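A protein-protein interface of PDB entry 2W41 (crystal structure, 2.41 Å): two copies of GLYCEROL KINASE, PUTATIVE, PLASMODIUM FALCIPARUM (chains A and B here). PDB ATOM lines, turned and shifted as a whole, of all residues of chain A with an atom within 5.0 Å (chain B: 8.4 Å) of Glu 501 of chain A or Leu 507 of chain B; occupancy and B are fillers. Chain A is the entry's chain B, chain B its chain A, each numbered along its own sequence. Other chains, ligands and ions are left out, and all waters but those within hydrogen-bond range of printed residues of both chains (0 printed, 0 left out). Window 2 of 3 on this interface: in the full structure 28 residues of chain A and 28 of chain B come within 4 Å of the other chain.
Arg 502 of chain A touches its own counterpart, Arg 502 of chain B. Arg 502 of chain A touches Thr 503 of chain B, and with the chains exchanged Thr 503 of chain A touches Arg 502 of chain B. Arg 502 of chain A touches Ile 505 of chain B, and with the chains exchanged Ile 505 of chain A touches Arg 502 of chain B. Of the 8 pairs that touch across the chains among the printed residues, 5 have their exchanged pair printed and touching as well.
The backbone carbonyl oxygen (O) of Ala 499 of chain A sits at hydrogen-bond distance from the side-chain hydroxyl (OG1) of Thr 503 of chain A, at 2.7 Å.
O of Arg 502 of chain B sits at hydrogen-bond distance from NH1 of Arg 502 of chain A, 2.7 Å away. NH1 of Arg 502 of chain B lies within hydrogen-bond range of O of Ile 505 of chain A (2.7 Å). The backbone carbonyl oxygen (O) of Ile 505 of chain B sits at hydrogen-bond distance from the guanidinium group (NH1) of Arg 502 of chain A (2.9 Å).
Lys 498 of chain A touches Leu 507 of chain B. Glu 501 of chain A touches Leu 507 of chain B (CB to CD1, 3.9 Å). NH1 of Arg 502 of chain A touches O of Thr 503 of chain B, at 3.7 Å. Leu 507 of chain B touches Arg 502 of chain A. Thr 503 of chain A touches Arg 502 of chain B.
Of chain B, only Leu 507 (3.9 Å) comes within 4 Å of Glu 501 of chain A. Of the printed residues of chain A, Leu 507 of chain B touches Lys 498 (3.5 Å), Glu 501 (3.9 Å) and Arg 502 (3.8 Å). Of the printed residues of chain B, Arg 502 of chain A touches Arg 502 (2.7 Å), Thr 503 (3.7 Å), Ile 505 (2.9 Å) and Leu 507 (3.8 Å). Of the printed residues of chain A, Ile 505 of chain B touches Arg 502. Printed residues of chain A within 4 Å of Thr 503 of chain B: Arg 502. The nearest residue of chain B that does not touch Glu 501 of chain A is Arg 502 of chain B (5.1 Å). The nearest printed residue of chain A that does not touch Leu 507 of chain B is Ala 499 of chain A (5.6 Å).
Hydrophobic or aromatic side chains of chain B within 4 Å of the printed part of chain A: Ile 505 and Leu 507. Printed residues of chain A that touch a printed residue of chain B: Lys 498, Glu 501, Arg 502, Thr 503 and Ile 505. Hydrophobic or aromatic side chains of chain A within 4 Å of the printed part of chain B: Ile 505. Along chain A the printed residues that touch a printed residue of chain B span positions 498 to 505.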
ATOM      1  N   ASN A 497      -9.397  21.704 -15.285  1.00  0.00           N
ATOM      2  CA  ASN A 497      -8.069  21.114 -15.205  1.00  0.00           C
ATOM      3  C   ASN A 497      -7.886  20.102 -14.078  1.00  0.00           C
ATOM      4  O   ASN A 497      -7.197  19.096 -14.263  1.00  0.00           O
ATOM      5  CB  ASN A 497      -6.994  22.205 -15.080  1.00  0.00           C
ATOM      6  CG  ASN A 497      -6.679  22.867 -16.393  1.00  0.00           C
ATOM      7  OD1 ASN A 497      -7.173  22.466 -17.445  1.00  0.00           O
ATOM      8  ND2 ASN A 497      -5.854  23.898 -16.342  1.00  0.00           N
ATOM      9  N   LYS A 498      -8.503  20.379 -12.931  1.00  0.00           N
ATOM     10  CA  LYS A 498      -8.433  19.509 -11.794  1.00  0.00           C
ATOM     11  C   LYS A 498      -9.280  18.274 -11.984  1.00  0.00           C
ATOM     12  O   LYS A 498      -8.936  17.203 -11.520  1.00  0.00           O
ATOM     13  CB  LYS A 498      -8.877  20.244 -10.534  1.00  0.00           C
ATOM     14  CG  LYS A 498      -7.831  21.208 -10.010  1.00  0.00           C
ATOM     15  CD  LYS A 498      -8.315  21.847  -8.703  1.00  0.00           C
ATOM     16  CE  LYS A 498      -7.540  23.123  -8.382  1.00  0.00           C
ATOM     17  NZ  LYS A 498      -8.358  24.019  -7.499  1.00  0.00           N
ATOM     18  N   ALA A 499     -10.430  18.455 -12.622  1.00  0.00           N
ATOM     19  CA  ALA A 499     -11.316  17.386 -12.959  1.00  0.00           C
ATOM     20  C   ALA A 499     -10.679  16.475 -14.011  1.00  0.00           C
ATOM     21  O   ALA A 499     -10.989  15.304 -14.065  1.00  0.00           O
ATOM     22  CB  ALA A 499     -12.612  17.952 -13.445  1.00  0.00           C
ATOM     23  N   VAL A 500      -9.817  17.016 -14.864  1.00  0.00           N
ATOM     24  CA  VAL A 500      -9.147  16.216 -15.890  1.00  0.00           C
ATOM     25  C   VAL A 500      -8.000  15.429 -15.240  1.00  0.00           C
ATOM     26  O   VAL A 500      -7.695  14.283 -15.596  1.00  0.00           O
ATOM     27  CB  VAL A 500      -8.663  17.082 -17.063  1.00  0.00           C
ATOM     28  CG1 VAL A 500      -7.698  16.311 -17.925  1.00  0.00           C
ATOM     29  CG2 VAL A 500      -9.836  17.583 -17.885  1.00  0.00           C
ATOM     30  N   GLU A 501      -7.428  16.033 -14.219  1.00  0.00           N
ATOM     31  CA  GLU A 501      -6.430  15.412 -13.381  1.00  0.00           C
ATOM     32  C   GLU A 501      -6.871  14.193 -12.598  1.00  0.00           C
ATOM     33  O   GLU A 501      -6.102  13.240 -12.478  1.00  0.00           O
ATOM     34  CB  GLU A 501      -6.048  16.437 -12.372  1.00  0.00           C
ATOM     35  CG  GLU A 501      -5.035  17.383 -12.863  1.00  0.00           C
ATOM     36  CD  GLU A 501      -3.729  16.977 -12.290  1.00  0.00           C
ATOM     37  OE1 GLU A 501      -3.260  15.863 -12.723  1.00  0.00           O
ATOM     38  OE2 GLU A 501      -3.256  17.736 -11.367  1.00  0.00           O
ATOM     39  N   ARG A 502      -8.055  14.266 -11.978  1.00  0.00           N
ATOM     40  CA  ARG A 502      -8.662  13.149 -11.275  1.00  0.00           C
ATOM     41  C   ARG A 502      -8.946  12.008 -12.241  1.00  0.00           C
ATOM     42  O   ARG A 502      -8.809  10.846 -11.905  1.00  0.00           O
ATOM     43  CB  ARG A 502     -10.022  13.553 -10.709  1.00  0.00           C
ATOM     44  CG  ARG A 502     -10.022  14.601  -9.671  1.00  0.00           C
ATOM     45  CD  ARG A 502     -11.386  14.718  -9.127  1.00  0.00           C
ATOM     46  NE  ARG A 502     -11.414  15.876  -8.262  1.00  0.00           N
ATOM     47  CZ  ARG A 502     -10.901  15.917  -7.033  1.00  0.00           C
ATOM     48  NH1 ARG A 502     -10.364  14.840  -6.476  1.00  0.00           N
ATOM     49  NH2 ARG A 502     -10.954  17.045  -6.340  1.00  0.00           N
ATOM     50  N   THR A 503      -9.408  12.388 -13.420  1.00  0.00           N
ATOM     51  CA  THR A 503      -9.705  11.497 -14.526  1.00  0.00           C
ATOM     52  C   THR A 503      -8.433  10.734 -15.028  1.00  0.00           C
ATOM     53  O   THR A 503      -8.524   9.580 -15.458  1.00  0.00           O
ATOM     54  CB  THR A 503     -10.394  12.339 -15.626  1.00  0.00           C
ATOM     55  OG1 THR A 503     -11.624  12.866 -15.097  1.00  0.00           O
ATOM     56  CG2 THR A 503     -10.631  11.571 -16.914  1.00  0.00           C
ATOM     57  N   LEU A 504      -7.268  11.376 -14.934  1.00  0.00           N
ATOM     58  CA  LEU A 504      -6.075  10.868 -15.579  1.00  0.00           C
ATOM     59  C   LEU A 504      -5.023  10.339 -14.609  1.00  0.00           C
ATOM     60  O   LEU A 504      -4.227   9.525 -14.985  1.00  0.00           O
ATOM     61  CB  LEU A 504      -5.451  11.929 -16.503  1.00  0.00           C
ATOM     62  CG  LEU A 504      -6.202  12.484 -17.709  1.00  0.00           C
ATOM     63  CD1 LEU A 504      -5.317  13.535 -18.376  1.00  0.00           C
ATOM     64  CD2 LEU A 504      -6.628  11.416 -18.725  1.00  0.00           C
ATOM     65  N   ILE A 505      -5.037  10.779 -13.361  1.00  0.00           N
ATOM     66  CA  ILE A 505      -4.037  10.361 -12.346  1.00  0.00           C
ATOM     67  C   ILE A 505      -3.954   8.838 -12.276  1.00  0.00           C
ATOM     68  O   ILE A 505      -4.990   8.148 -12.352  1.00  0.00           O
ATOM     69  CB  ILE A 505      -4.350  10.976 -10.955  1.00  0.00           C
ATOM     70  CG1 ILE A 505      -3.278  10.644  -9.908  1.00  0.00           C
ATOM     71  CG2 ILE A 505      -5.694  10.510 -10.454  1.00  0.00           C
ATOM     72  CD1 ILE A 505      -2.317  11.814  -9.532  1.00  0.00           C
ATOM     73  N   ARG B 365     -15.447  11.866   5.200  1.00  0.00           N
ATOM     74  CA  ARG B 365     -15.131  12.951   4.266  1.00  0.00           C
ATOM     75  C   ARG B 365     -16.408  13.682   3.753  1.00  0.00           C
ATOM     76  O   ARG B 365     -17.038  13.257   2.757  1.00  0.00           O
ATOM     77  CB  ARG B 365     -14.270  12.394   3.129  1.00  0.00           C
ATOM     78  CG  ARG B 365     -12.889  11.944   3.615  1.00  0.00           C
ATOM     79  CD  ARG B 365     -11.938  13.158   3.939  1.00  0.00           C
ATOM     80  NE  ARG B 365     -11.694  14.007   2.770  1.00  0.00           N
ATOM     81  CZ  ARG B 365     -10.625  13.897   1.967  1.00  0.00           C
ATOM     82  NH1 ARG B 365      -9.686  12.970   2.216  1.00  0.00           N
ATOM     83  NH2 ARG B 365     -10.485  14.709   0.894  1.00  0.00           N
ATOM     84  N   GLU B 501     -10.247   7.172  -4.149  1.00  0.00           N
ATOM     85  CA  GLU B 501      -9.064   7.994  -4.152  1.00  0.00           C
ATOM     86  C   GLU B 501      -9.134   9.190  -5.098  1.00  0.00           C
ATOM     87  O   GLU B 501      -8.697  10.284  -4.721  1.00  0.00           O
ATOM     88  CB  GLU B 501      -7.935   7.127  -4.615  1.00  0.00           C
ATOM     89  CG  GLU B 501      -7.332   6.343  -3.533  1.00  0.00           C
ATOM     90  CD  GLU B 501      -6.017   6.968  -3.208  1.00  0.00           C
ATOM     91  OE1 GLU B 501      -6.052   8.124  -2.635  1.00  0.00           O
ATOM     92  OE2 GLU B 501      -4.984   6.336  -3.607  1.00  0.00           O
ATOM     93  N   ARG B 502      -9.617   8.957  -6.332  1.00  0.00           N
ATOM     94  CA  ARG B 502      -9.789   9.994  -7.329  1.00  0.00           C
ATOM     95  C   ARG B 502     -10.767  11.041  -6.831  1.00  0.00           C
ATOM     96  O   ARG B 502     -10.597  12.219  -7.066  1.00  0.00           O
ATOM     97  CB  ARG B 502     -10.391   9.414  -8.608  1.00  0.00           C
ATOM     98  CG  ARG B 502      -9.542   8.453  -9.347  1.00  0.00           C
ATOM     99  CD  ARG B 502     -10.135   8.214 -10.650  1.00  0.00           C
ATOM    100  NE  ARG B 502      -9.436   7.097 -11.245  1.00  0.00           N
ATOM    101  CZ  ARG B 502      -8.274   7.198 -11.876  1.00  0.00           C
ATOM    102  NH1 ARG B 502      -7.683   8.373 -12.035  1.00  0.00           N
ATOM    103  NH2 ARG B 502      -7.711   6.119 -12.375  1.00  0.00           N
ATOM    104  N   THR B 503     -11.811  10.545  -6.180  1.00  0.00           N
ATOM    105  CA  THR B 503     -12.897  11.291  -5.588  1.00  0.00           C
ATOM    106  C   THR B 503     -12.410  12.208  -4.448  1.00  0.00           C
ATOM    107  O   THR B 503     -12.919  13.327  -4.301  1.00  0.00           O
ATOM    108  CB  THR B 503     -13.980  10.255  -5.116  1.00  0.00           C
ATOM    109  OG1 THR B 503     -14.503   9.573  -6.269  1.00  0.00           O
ATOM    110  CG2 THR B 503     -15.107  10.873  -4.266  1.00  0.00           C
ATOM    111  N   LEU B 504     -11.412  11.740  -3.686  1.00  0.00           N
ATOM    112  CA  LEU B 504     -10.926  12.439  -2.502  1.00  0.00           C
ATOM    113  C   LEU B 504      -9.592  13.178  -2.643  1.00  0.00           C
ATOM    114  O   LEU B 504      -9.342  14.063  -1.878  1.00  0.00           O
ATOM    115  CB  LEU B 504     -10.850  11.477  -1.309  1.00  0.00           C
ATOM    116  CG  LEU B 504     -12.081  10.683  -0.872  1.00  0.00           C
ATOM    117  CD1 LEU B 504     -11.694   9.703   0.237  1.00  0.00           C
ATOM    118  CD2 LEU B 504     -13.233  11.586  -0.421  1.00  0.00           C
ATOM    119  N   ILE B 505      -8.728  12.818  -3.593  1.00  0.00           N
ATOM    120  CA  ILE B 505      -7.373  13.431  -3.749  1.00  0.00           C
ATOM    121  C   ILE B 505      -7.509  14.960  -3.802  1.00  0.00           C
ATOM    122  O   ILE B 505      -8.441  15.484  -4.440  1.00  0.00           O
ATOM    123  CB  ILE B 505      -6.633  12.884  -5.016  1.00  0.00           C
ATOM    124  CG1 ILE B 505      -5.178  13.383  -5.125  1.00  0.00           C
ATOM    125  CG2 ILE B 505      -7.393  13.214  -6.296  1.00  0.00           C
ATOM    126  CD1 ILE B 505      -4.078  12.338  -4.703  1.00  0.00           C
ATOM    127  N   GLN B 506      -6.607  15.666  -3.113  1.00  0.00           N
ATOM    128  CA  GLN B 506      -6.714  17.143  -2.968  1.00  0.00           C
ATOM    129  C   GLN B 506      -5.832  17.842  -3.972  1.00  0.00           C
ATOM    130  O   GLN B 506      -4.658  17.525  -4.083  1.00  0.00           O
ATOM    131  CB  GLN B 506      -6.463  17.601  -1.511  1.00  0.00           C
ATOM    132  CG  GLN B 506      -7.508  17.030  -0.587  1.00  0.00           C
ATOM    133  CD  GLN B 506      -7.499  17.629   0.785  1.00  0.00           C
ATOM    134  OE1 GLN B 506      -7.140  16.953   1.765  1.00  0.00           O
ATOM    135  NE2 GLN B 506      -7.922  18.904   0.895  1.00  0.00           N
ATOM    136  N   LEU B 507      -6.425  18.748  -4.749  1.00  0.00           N
ATOM    137  CA  LEU B 507      -5.722  19.309  -5.915  1.00  0.00           C
ATOM    138  C   LEU B 507      -5.852  20.832  -6.006  1.00  0.00           C
ATOM    139  O   LEU B 507      -6.520  21.446  -5.167  1.00  0.00           O
ATOM    140  CB  LEU B 507      -6.189  18.622  -7.211  1.00  0.00           C
ATOM    141  CG  LEU B 507      -6.154  17.092  -7.416  1.00  0.00           C
ATOM    142  CD1 LEU B 507      -7.070  16.651  -8.579  1.00  0.00           C
ATOM    143  CD2 LEU B 507      -4.741  16.526  -7.624  1.00  0.00           C
